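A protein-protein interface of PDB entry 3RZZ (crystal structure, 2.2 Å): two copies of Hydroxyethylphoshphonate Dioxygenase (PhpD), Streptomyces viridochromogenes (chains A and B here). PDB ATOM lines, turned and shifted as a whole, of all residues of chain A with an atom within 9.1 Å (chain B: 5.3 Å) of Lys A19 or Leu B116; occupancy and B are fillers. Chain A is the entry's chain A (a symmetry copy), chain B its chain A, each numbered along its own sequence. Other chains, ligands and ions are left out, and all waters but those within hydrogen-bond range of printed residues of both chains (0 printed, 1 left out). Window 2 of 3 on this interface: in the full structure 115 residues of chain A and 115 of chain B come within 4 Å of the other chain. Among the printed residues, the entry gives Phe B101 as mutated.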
ATOM      1  N   LEU A  11      -1.212  37.326  24.801  1.00  0.00           N
ATOM      2  CA  LEU A  11      -0.656  36.071  24.304  1.00  0.00           C
ATOM      3  C   LEU A  11      -1.758  35.128  23.818  1.00  0.00           C
ATOM      4  O   LEU A  11      -1.650  34.527  22.750  1.00  0.00           O
ATOM      5  CB  LEU A  11       0.166  35.383  25.403  1.00  0.00           C
ATOM      6  CG  LEU A  11       0.790  34.031  25.033  1.00  0.00           C
ATOM      7  CD1 LEU A  11       1.815  34.219  23.913  1.00  0.00           C
ATOM      8  CD2 LEU A  11       1.449  33.425  26.249  1.00  0.00           C
ATOM      9  N   ALA A  12      -2.812  34.995  24.615  1.00  0.00           N
ATOM     10  CA  ALA A  12      -3.926  34.136  24.251  1.00  0.00           C
ATOM     11  C   ALA A  12      -4.554  34.663  22.963  1.00  0.00           C
ATOM     12  O   ALA A  12      -4.978  33.889  22.102  1.00  0.00           O
ATOM     13  CB  ALA A  12      -4.954  34.117  25.370  1.00  0.00           C
ATOM     14  N   HIS A  13      -4.596  35.986  22.835  1.00  0.00           N
ATOM     15  CA  HIS A  13      -5.166  36.631  21.661  1.00  0.00           C
ATOM     16  C   HIS A  13      -4.366  36.315  20.403  1.00  0.00           C
ATOM     17  O   HIS A  13      -4.941  36.045  19.349  1.00  0.00           O
ATOM     18  CB  HIS A  13      -5.224  38.148  21.875  1.00  0.00           C
ATOM     19  CG  HIS A  13      -5.248  38.942  20.609  1.00  0.00           C
ATOM     20  ND1 HIS A  13      -6.295  38.887  19.711  1.00  0.00           N
ATOM     21  CD2 HIS A  13      -4.332  39.777  20.064  1.00  0.00           C
ATOM     22  CE1 HIS A  13      -6.020  39.652  18.669  1.00  0.00           C
ATOM     23  NE2 HIS A  13      -4.834  40.202  18.857  1.00  0.00           N
ATOM     24  N   TRP A  14      -3.040  36.346  20.516  1.00  0.00           N
ATOM     25  CA  TRP A  14      -2.176  36.082  19.369  1.00  0.00           C
ATOM     26  C   TRP A  14      -2.038  34.616  19.005  1.00  0.00           C
ATOM     27  O   TRP A  14      -1.836  34.282  17.836  1.00  0.00           O
ATOM     28  CB  TRP A  14      -0.802  36.713  19.583  1.00  0.00           C
ATOM     29  CG  TRP A  14      -0.828  38.169  19.253  1.00  0.00           C
ATOM     30  CD1 TRP A  14      -0.495  39.208  20.071  1.00  0.00           C
ATOM     31  CD2 TRP A  14      -1.260  38.749  18.018  1.00  0.00           C
ATOM     32  NE1 TRP A  14      -0.698  40.399  19.425  1.00  0.00           N
ATOM     33  CE2 TRP A  14      -1.168  40.147  18.161  1.00  0.00           C
ATOM     34  CE3 TRP A  14      -1.717  38.220  16.803  1.00  0.00           C
ATOM     35  CZ2 TRP A  14      -1.518  41.031  17.132  1.00  0.00           C
ATOM     36  CZ3 TRP A  14      -2.065  39.092  15.782  1.00  0.00           C
ATOM     37  CH2 TRP A  14      -1.963  40.485  15.954  1.00  0.00           C
ATOM     38  N   MET A  15      -2.133  33.739  19.996  1.00  0.00           N
ATOM     39  CA  MET A  15      -2.066  32.315  19.709  1.00  0.00           C
ATOM     40  C   MET A  15      -3.376  31.992  18.994  1.00  0.00           C
ATOM     41  O   MET A  15      -3.398  31.219  18.040  1.00  0.00           O
ATOM     42  CB  MET A  15      -1.958  31.496  20.995  1.00  0.00           C
ATOM     43  CG  MET A  15      -0.571  31.452  21.606  1.00  0.00           C
ATOM     44  SD  MET A  15      -0.600  30.644  23.220  1.00  0.00           S
ATOM     45  CE  MET A  15      -1.118  28.995  22.775  1.00  0.00           C
ATOM     46  N   ASN A  16      -4.463  32.605  19.460  1.00  0.00           N
ATOM     47  CA  ASN A  16      -5.778  32.397  18.863  1.00  0.00           C
ATOM     48  C   ASN A  16      -5.802  32.953  17.439  1.00  0.00           C
ATOM     49  O   ASN A  16      -6.297  32.303  16.520  1.00  0.00           O
ATOM     50  CB  ASN A  16      -6.864  33.093  19.685  1.00  0.00           C
ATOM     51  CG  ASN A  16      -8.237  32.995  19.032  1.00  0.00           C
ATOM     52  OD1 ASN A  16      -8.835  31.912  18.960  1.00  0.00           O
ATOM     53  ND2 ASN A  16      -8.737  34.123  18.538  1.00  0.00           N
ATOM     54  N   ALA A  17      -5.274  34.161  17.270  1.00  0.00           N
ATOM     55  CA  ALA A  17      -5.232  34.797  15.959  1.00  0.00           C
ATOM     56  C   ALA A  17      -4.538  33.883  14.961  1.00  0.00           C
ATOM     57  O   ALA A  17      -5.101  33.523  13.926  1.00  0.00           O
ATOM     58  CB  ALA A  17      -4.492  36.122  16.045  1.00  0.00           C
ATOM     59  N   ARG A  18      -3.306  33.514  15.281  1.00  0.00           N
ATOM     60  CA  ARG A  18      -2.515  32.643  14.426  1.00  0.00           C
ATOM     61  C   ARG A  18      -3.007  31.206  14.551  1.00  0.00           C
ATOM     62  O   ARG A  18      -2.480  30.303  13.904  1.00  0.00           O
ATOM     63  CB  ARG A  18      -1.050  32.714  14.854  1.00  0.00           C
ATOM     64  CG  ARG A  18      -0.464  34.119  14.845  1.00  0.00           C
ATOM     65  CD  ARG A  18      -0.274  34.618  13.429  1.00  0.00           C
ATOM     66  NE  ARG A  18       0.432  35.888  13.398  1.00  0.00           N
ATOM     67  CZ  ARG A  18      -0.154  37.079  13.323  1.00  0.00           C
ATOM     68  NH1 ARG A  18      -1.474  37.180  13.268  1.00  0.00           N
ATOM     69  NH2 ARG A  18       0.590  38.174  13.302  1.00  0.00           N
ATOM     70  N   LYS A  19      -4.031  31.020  15.380  1.00  0.00           N
ATOM     71  CA  LYS A  19      -4.612  29.713  15.687  1.00  0.00           C
ATOM     72  C   LYS A  19      -3.593  28.582  15.854  1.00  0.00           C
ATOM     73  O   LYS A  19      -3.636  27.559  15.171  1.00  0.00           O
ATOM     74  CB  LYS A  19      -5.702  29.321  14.682  1.00  0.00           C
ATOM     75  CG  LYS A  19      -5.306  29.269  13.236  1.00  0.00           C
ATOM     76  CD  LYS A  19      -6.522  28.914  12.388  1.00  0.00           C
ATOM     77  CE  LYS A  19      -7.643  29.937  12.567  1.00  0.00           C
ATOM     78  NZ  LYS A  19      -8.860  29.619  11.769  1.00  0.00           N
ATOM     79  N   TYR A  20      -2.675  28.800  16.788  1.00  0.00           N
ATOM     80  CA  TYR A  20      -1.641  27.835  17.138  1.00  0.00           C
ATOM     81  C   TYR A  20      -2.055  27.253  18.480  1.00  0.00           C
ATOM     82  O   TYR A  20      -2.474  27.994  19.372  1.00  0.00           O
ATOM     83  CB  TYR A  20      -0.291  28.533  17.318  1.00  0.00           C
ATOM     84  CG  TYR A  20       0.435  28.884  16.044  1.00  0.00           C
ATOM     85  CD1 TYR A  20       1.196  30.049  15.959  1.00  0.00           C
ATOM     86  CD2 TYR A  20       0.413  28.028  14.940  1.00  0.00           C
ATOM     87  CE1 TYR A  20       1.923  30.358  14.809  1.00  0.00           C
ATOM     88  CE2 TYR A  20       1.139  28.326  13.783  1.00  0.00           C
ATOM     89  CZ  TYR A  20       1.893  29.494  13.726  1.00  0.00           C
ATOM     90  OH  TYR A  20       2.626  29.791  12.597  1.00  0.00           O
ATOM     91  N   THR A  21      -1.949  25.938  18.631  1.00  0.00           N
ATOM     92  CA  THR A  21      -2.301  25.319  19.903  1.00  0.00           C
ATOM     93  C   THR A  21      -1.158  25.634  20.861  1.00  0.00           C
ATOM     94  O   THR A  21      -0.110  26.123  20.432  1.00  0.00           O
ATOM     95  CB  THR A  21      -2.444  23.787  19.781  1.00  0.00           C
ATOM     96  OG1 THR A  21      -3.102  23.277  20.948  1.00  0.00           O
ATOM     97  CG2 THR A  21      -1.080  23.129  19.672  1.00  0.00           C
ATOM     98  N   ALA A  22      -1.355  25.366  22.150  1.00  0.00           N
ATOM     99  CA  ALA A  22      -0.316  25.630  23.143  1.00  0.00           C
ATOM    100  C   ALA A  22       0.969  24.867  22.804  1.00  0.00           C
ATOM    101  O   ALA A  22       2.074  25.408  22.905  1.00  0.00           O
ATOM    102  CB  ALA A  22      -0.808  25.238  24.527  1.00  0.00           C
ATOM    103  N   GLN A  24       1.863  23.687  19.790  1.00  0.00           N
ATOM    104  CA  GLN A  24       2.410  24.215  18.549  1.00  0.00           C
ATOM    105  C   GLN A  24       3.143  25.511  18.824  1.00  0.00           C
ATOM    106  O   GLN A  24       4.164  25.805  18.204  1.00  0.00           O
ATOM    107  CB  GLN A  24       1.291  24.474  17.536  1.00  0.00           C
ATOM    108  CG  GLN A  24       0.691  23.217  16.932  1.00  0.00           C
ATOM    109  CD  GLN A  24      -0.523  23.506  16.064  1.00  0.00           C
ATOM    110  OE1 GLN A  24      -1.550  23.983  16.549  1.00  0.00           O
ATOM    111  NE2 GLN A  24      -0.406  23.217  14.773  1.00  0.00           N
ATOM    112  N   THR A  25       2.614  26.292  19.758  1.00  0.00           N
ATOM    113  CA  THR A  25       3.230  27.564  20.115  1.00  0.00           C
ATOM    114  C   THR A  25       4.590  27.308  20.758  1.00  0.00           C
ATOM    115  O   THR A  25       5.594  27.900  20.362  1.00  0.00           O
ATOM    116  CB  THR A  25       2.336  28.364  21.096  1.00  0.00           C
ATOM    117  OG1 THR A  25       1.062  28.604  20.489  1.00  0.00           O
ATOM    118  CG2 THR A  25       2.972  29.699  21.439  1.00  0.00           C
ATOM    119  N   ALA A  58       7.795  33.581  16.954  1.00  0.00           N
ATOM    120  CA  ALA A  58       6.906  32.493  16.560  1.00  0.00           C
ATOM    121  C   ALA A  58       5.487  32.957  16.241  1.00  0.00           C
ATOM    122  O   ALA A  58       4.762  32.283  15.518  1.00  0.00           O
ATOM    123  CB  ALA A  58       6.875  31.432  17.647  1.00  0.00           C
ATOM    124  N   LEU A  59       5.092  34.109  16.777  1.00  0.00           N
ATOM    125  CA  LEU A  59       3.750  34.632  16.543  1.00  0.00           C
ATOM    126  C   LEU A  59       3.702  35.763  15.516  1.00  0.00           C
ATOM    127  O   LEU A  59       2.649  36.354  15.287  1.00  0.00           O
ATOM    128  CB  LEU A  59       3.137  35.093  17.868  1.00  0.00           C
ATOM    129  CG  LEU A  59       2.785  33.925  18.794  1.00  0.00           C
ATOM    130  CD1 LEU A  59       2.499  34.424  20.186  1.00  0.00           C
ATOM    131  CD2 LEU A  59       1.592  33.175  18.224  1.00  0.00           C
ATOM    132  N   ARG B  89      -2.719  24.694   6.047  1.00  0.00           N
ATOM    133  CA  ARG B  89      -2.288  24.067   7.287  1.00  0.00           C
ATOM    134  C   ARG B  89      -3.444  23.268   7.868  1.00  0.00           C
ATOM    135  O   ARG B  89      -4.546  23.791   8.025  1.00  0.00           O
ATOM    136  CB  ARG B  89      -1.831  25.125   8.290  1.00  0.00           C
ATOM    137  CG  ARG B  89      -0.361  25.046   8.658  1.00  0.00           C
ATOM    138  CD  ARG B  89      -0.075  25.820   9.932  1.00  0.00           C
ATOM    139  NE  ARG B  89      -0.947  25.409  11.027  1.00  0.00           N
ATOM    140  CZ  ARG B  89      -1.553  26.251  11.856  1.00  0.00           C
ATOM    141  NH1 ARG B  89      -1.384  27.559  11.718  1.00  0.00           N
ATOM    142  NH2 ARG B  89      -2.329  25.788  12.826  1.00  0.00           N
ATOM    143  N   ILE B  91      -5.682  21.289  10.669  1.00  0.00           N
ATOM    144  CA  ILE B  91      -5.895  21.374  12.102  1.00  0.00           C
ATOM    145  C   ILE B  91      -6.615  20.086  12.482  1.00  0.00           C
ATOM    146  O   ILE B  91      -7.620  19.707  11.868  1.00  0.00           O
ATOM    147  CB  ILE B  91      -6.732  22.625  12.541  1.00  0.00           C
ATOM    148  CG1 ILE B  91      -8.230  22.354  12.407  1.00  0.00           C
ATOM    149  CG2 ILE B  91      -6.312  23.849  11.746  1.00  0.00           C
ATOM    150  CD1 ILE B  91      -8.844  21.705  13.646  1.00  0.00           C
ATOM    151  N   TYR B  99     -10.143  20.698   9.901  1.00  0.00           N
ATOM    152  CA  TYR B  99     -10.133  21.826   8.974  1.00  0.00           C
ATOM    153  C   TYR B  99      -8.826  21.906   8.195  1.00  0.00           C
ATOM    154  O   TYR B  99      -7.835  21.264   8.548  1.00  0.00           O
ATOM    155  CB  TYR B  99     -10.262  23.169   9.718  1.00  0.00           C
ATOM    156  CG  TYR B  99     -11.540  23.442  10.492  1.00  0.00           C
ATOM    157  CD1 TYR B  99     -12.795  23.368   9.877  1.00  0.00           C
ATOM    158  CD2 TYR B  99     -11.482  23.868  11.820  1.00  0.00           C
ATOM    159  CE1 TYR B  99     -13.960  23.719  10.569  1.00  0.00           C
ATOM    160  CE2 TYR B  99     -12.631  24.222  12.516  1.00  0.00           C
ATOM    161  CZ  TYR B  99     -13.868  24.148  11.888  1.00  0.00           C
ATOM    162  OH  TYR B  99     -15.003  24.515  12.582  1.00  0.00           O
ATOM    163  N   ASN B 100      -8.835  22.730   7.152  1.00  0.00           N
ATOM    164  CA  ASN B 100      -7.632  23.098   6.421  1.00  0.00           C
ATOM    165  C   ASN B 100      -7.448  24.608   6.520  1.00  0.00           C
ATOM    166  O   ASN B 100      -8.322  25.373   6.114  1.00  0.00           O
ATOM    167  CB  ASN B 100      -7.729  22.665   4.960  1.00  0.00           C
ATOM    168  CG  ASN B 100      -6.952  21.395   4.675  1.00  0.00           C
ATOM    169  OD1 ASN B 100      -6.044  21.029   5.420  1.00  0.00           O
ATOM    170  ND2 ASN B 100      -7.306  20.715   3.592  1.00  0.00           N
ATOM    171  N   PHE B 101      -6.319  25.034   7.077  1.00  0.00           N
ATOM    172  CA  PHE B 101      -6.091  26.448   7.360  1.00  0.00           C
ATOM    173  C   PHE B 101      -5.394  27.204   6.229  1.00  0.00           C
ATOM    174  O   PHE B 101      -4.312  26.822   5.785  1.00  0.00           O
ATOM    175  CB  PHE B 101      -5.295  26.604   8.659  1.00  0.00           C
ATOM    176  CG  PHE B 101      -5.282  28.004   9.200  1.00  0.00           C
ATOM    177  CD1 PHE B 101      -4.194  28.473   9.917  1.00  0.00           C
ATOM    178  CD2 PHE B 101      -6.356  28.851   8.992  1.00  0.00           C
ATOM    179  CE1 PHE B 101      -4.179  29.761  10.415  1.00  0.00           C
ATOM    180  CE2 PHE B 101      -6.347  30.140   9.488  1.00  0.00           C
ATOM    181  CZ  PHE B 101      -5.255  30.594  10.201  1.00  0.00           C
ATOM    182  N   TYR B 102      -6.025  28.284   5.779  1.00  0.00           N
ATOM    183  CA  TYR B 102      -5.450  29.160   4.765  1.00  0.00           C
ATOM    184  C   TYR B 102      -5.523  30.608   5.238  1.00  0.00           C
ATOM    185  O   TYR B 102      -6.455  30.987   5.945  1.00  0.00           O
ATOM    186  CB  TYR B 102      -6.201  29.024   3.439  1.00  0.00           C
ATOM    187  CG  TYR B 102      -6.293  27.613   2.905  1.00  0.00           C
ATOM    188  CD1 TYR B 102      -5.314  27.104   2.065  1.00  0.00           C
ATOM    189  CD2 TYR B 102      -7.368  26.798   3.230  1.00  0.00           C
ATOM    190  CE1 TYR B 102      -5.397  25.817   1.570  1.00  0.00           C
ATOM    191  CE2 TYR B 102      -7.460  25.510   2.740  1.00  0.00           C
ATOM    192  CZ  TYR B 102      -6.473  25.025   1.911  1.00  0.00           C
ATOM    193  OH  TYR B 102      -6.562  23.743   1.421  1.00  0.00           O
ATOM    194  N   VAL B 114      -9.218  34.432   7.227  1.00  0.00           N
ATOM    195  CA  VAL B 114      -8.980  33.005   7.047  1.00  0.00           C
ATOM    196  C   VAL B 114      -9.989  32.259   6.180  1.00  0.00           C
ATOM    197  O   VAL B 114     -11.192  32.517   6.237  1.00  0.00           O
ATOM    198  CB  VAL B 114      -8.900  32.316   8.430  1.00  0.00           C
ATOM    199  CG1 VAL B 114      -9.835  33.014   9.387  1.00  0.00           C
ATOM    200  CG2 VAL B 114      -9.298  30.858   8.332  1.00  0.00           C
ATOM    201  N   VAL B 115      -9.479  31.337   5.368  1.00  0.00           N
ATOM    202  CA  VAL B 115     -10.323  30.494   4.527  1.00  0.00           C
ATOM    203  C   VAL B 115     -10.181  29.114   5.144  1.00  0.00           C
ATOM    204  O   VAL B 115      -9.085  28.711   5.510  1.00  0.00           O
ATOM    205  CB  VAL B 115      -9.845  30.446   3.056  1.00  0.00           C
ATOM    206  CG1 VAL B 115     -10.660  29.419   2.267  1.00  0.00           C
ATOM    207  CG2 VAL B 115      -9.997  31.810   2.415  1.00  0.00           C
ATOM    208  N   LEU B 116     -11.288  28.397   5.287  1.00  0.00           N
ATOM    209  CA  LEU B 116     -11.238  27.073   5.880  1.00  0.00           C
ATOM    210  C   LEU B 116     -11.908  26.005   5.044  1.00  0.00           C
ATOM    211  O   LEU B 116     -12.972  26.229   4.472  1.00  0.00           O
ATOM    212  CB  LEU B 116     -11.923  27.060   7.248  1.00  0.00           C
ATOM    213  CG  LEU B 116     -11.351  27.742   8.491  1.00  0.00           C
ATOM    214  CD1 LEU B 116     -12.305  27.458   9.641  1.00  0.00           C
ATOM    215  CD2 LEU B 116      -9.958  27.208   8.828  1.00  0.00           C
ATOM    216  N   ASP B 117     -11.267  24.846   4.965  1.00  0.00           N
ATOM    217  CA  ASP B 117     -11.878  23.717   4.287  1.00  0.00           C
ATOM    218  C   ASP B 117     -12.671  23.084   5.432  1.00  0.00           C
ATOM    219  O   ASP B 117     -12.176  23.001   6.554  1.00  0.00           O
ATOM    220  CB  ASP B 117     -10.832  22.712   3.790  1.00  0.00           C
ATOM    221  CG  ASP B 117     -10.309  23.037   2.401  1.00  0.00           C
ATOM    222  OD1 ASP B 117     -11.136  23.218   1.477  1.00  0.00           O
ATOM    223  OD2 ASP B 117      -9.071  23.094   2.228  1.00  0.00           O
ATOM    224  N   ILE B 118     -13.902  22.671   5.165  1.00  0.00           N
ATOM    225  CA  ILE B 118     -14.714  22.021   6.185  1.00  0.00           C
ATOM    226  C   ILE B 118     -14.573  20.515   5.913  1.00  0.00           C
ATOM    227  O   ILE B 118     -15.130  19.998   4.936  1.00  0.00           O
ATOM    228  CB  ILE B 118     -16.191  22.452   6.073  1.00  0.00           C
ATOM    229  CG1 ILE B 118     -16.283  23.989   6.043  1.00  0.00           C
ATOM    230  CG2 ILE B 118     -16.993  21.851   7.220  1.00  0.00           C
ATOM    231  CD1 ILE B 118     -15.728  24.703   7.294  1.00  0.00           C
ATOM    232  N   ALA B 195     -16.878  21.802   0.908  1.00  0.00           N
ATOM    233  CA  ALA B 195     -17.209  23.201   1.138  1.00  0.00           C
ATOM    234  C   ALA B 195     -16.100  23.971   1.822  1.00  0.00           C
ATOM    235  O   ALA B 195     -15.333  23.419   2.621  1.00  0.00           O
ATOM    236  CB  ALA B 195     -18.486  23.305   1.968  1.00  0.00           C
ATOM    237  N   ARG B 196     -16.018  25.254   1.494  1.00  0.00           N
ATOM    238  CA  ARG B 196     -15.031  26.136   2.095  1.00  0.00           C
ATOM    239  C   ARG B 196     -15.741  27.309   2.720  1.00  0.00           C
ATOM    240  O   ARG B 196     -16.831  27.704   2.292  1.00  0.00           O
ATOM    241  CB  ARG B 196     -14.035  26.663   1.064  1.00  0.00           C
ATOM    242  CG  ARG B 196     -13.049  25.634   0.601  1.00  0.00           C
ATOM    243  CD  ARG B 196     -11.916  26.312  -0.106  1.00  0.00           C
ATOM    244  NE  ARG B 196     -12.368  27.068  -1.270  1.00  0.00           N
ATOM    245  CZ  ARG B 196     -11.613  27.957  -1.900  1.00  0.00           C
ATOM    246  NH1 ARG B 196     -10.379  28.197  -1.476  1.00  0.00           N
ATOM    247  NH2 ARG B 196     -12.087  28.612  -2.949  1.00  0.00           N
ATOM    248  N   ILE B 197     -15.101  27.875   3.732  1.00  0.00           N
ATOM    249  CA  ILE B 197     -15.659  29.009   4.433  1.00  0.00           C
ATOM    250  C   ILE B 197     -14.636  30.127   4.525  1.00  0.00           C
ATOM    251  O   ILE B 197     -13.428  29.877   4.535  1.00  0.00           O
ATOM    252  CB  ILE B 197     -16.110  28.573   5.852  1.00  0.00           C
ATOM    253  CG1 ILE B 197     -17.540  29.025   6.075  1.00  0.00           C
ATOM    254  CG2 ILE B 197     -15.177  29.106   6.925  1.00  0.00           C
ATOM    255  CD1 ILE B 197     -18.481  28.342   5.149  1.00  0.00           C
ATOM    256  N   VAL B 198     -15.133  31.359   4.541  1.00  0.00           N
ATOM    257  CA  VAL B 198     -14.296  32.538   4.705  1.00  0.00           C
ATOM    258  C   VAL B 198     -14.776  33.134   6.023  1.00  0.00           C
ATOM    259  O   VAL B 198     -15.967  33.365   6.200  1.00  0.00           O
ATOM    260  CB  VAL B 198     -14.511  33.588   3.595  1.00  0.00           C
ATOM    261  CG1 VAL B 198     -13.985  34.920   4.060  1.00  0.00           C
ATOM    262  CG2 VAL B 198     -13.779  33.178   2.329  1.00  0.00           C
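Among the printed residues, merely in contact across the chains: Lys A19 with Phe B101, Tyr A20 with Arg B89, Arg A18 with Arg B89, Lys A19 with Val B114, Gln A24 with Arg B89, Arg A18 with Phe B101 and Lys A19 with Leu B116.
NH2 of Arg B89 is in hydrogen-bond range of O of Lys A19 (3.2 Å).
Of the 16 printed residues of chain A, 4 touch a printed residue of chain B. Hydrophobic or aromatic side chains of chain A within 4 Å of the printed part of chain B: Tyr A20. Of the 15 printed residues of chain B, 4 touch a printed residue of chain A. Among the printed residues, 8 pairs touch across the chains.
Ala A12 touches none of the printed residues of chain B. Of the printed residues of chain B, Arg A18 touches Arg B89 and Phe B101. Lys A19 touches just these residues of chain B: Arg B89 (3.2 Å), Phe B101 (3.0 Å), Val B114 (3.7 Å) and Leu B116 (3.96 Å). Of the printed residues of chain B, Gln A24 touches Arg B89. Of the printed residues of chain A, Arg B89 touches Arg A18, Lys A19, Tyr A20 and Gln A24. Asn B100 touches none of the printed residues of chain A. Of the printed residues of chain A, Phe B101 touches Arg A18 (3.9 Å) and Lys A19 (3.0 Å). Of the printed residues of chain A, Val B114 touches Lys A19 (3.7 Å). Leu B116 touches just one residue of chain A: Lys A19 (3.96 Å). No residue of chain A comes within 4 Å of Asp B117. The nearest residue of chain B that does not touch Lys A19 is Ile B91 (5.1 Å). The nearest printed residue of chain A that does not touch Leu B116 is Ala A17 (9.5 Å).
No position is printed for both chains. Of the 8 pairs that touch across the chains among the printed residues, none has its exchanged pair printed and touching as well.
The backbone carbonyl oxygen (O) of Phe B101 sits at hydrogen-bond distance from the backbone NH (N) of Arg B89 (2.7 Å). The backbone NH (N) of Leu B116 is in hydrogen-bond range of the backbone carbonyl oxygen (O) of Ile B197, at 2.7 Å. The backbone NH (N) of Tyr A20 lies within hydrogen-bond range of the backbone carbonyl oxygen (O) of Met A15, at 2.8 Å. O of Leu A59 sits at hydrogen-bond distance from NE of Arg A18. N of Thr A21 sits at hydrogen-bond distance from OE1 of Gln A24.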
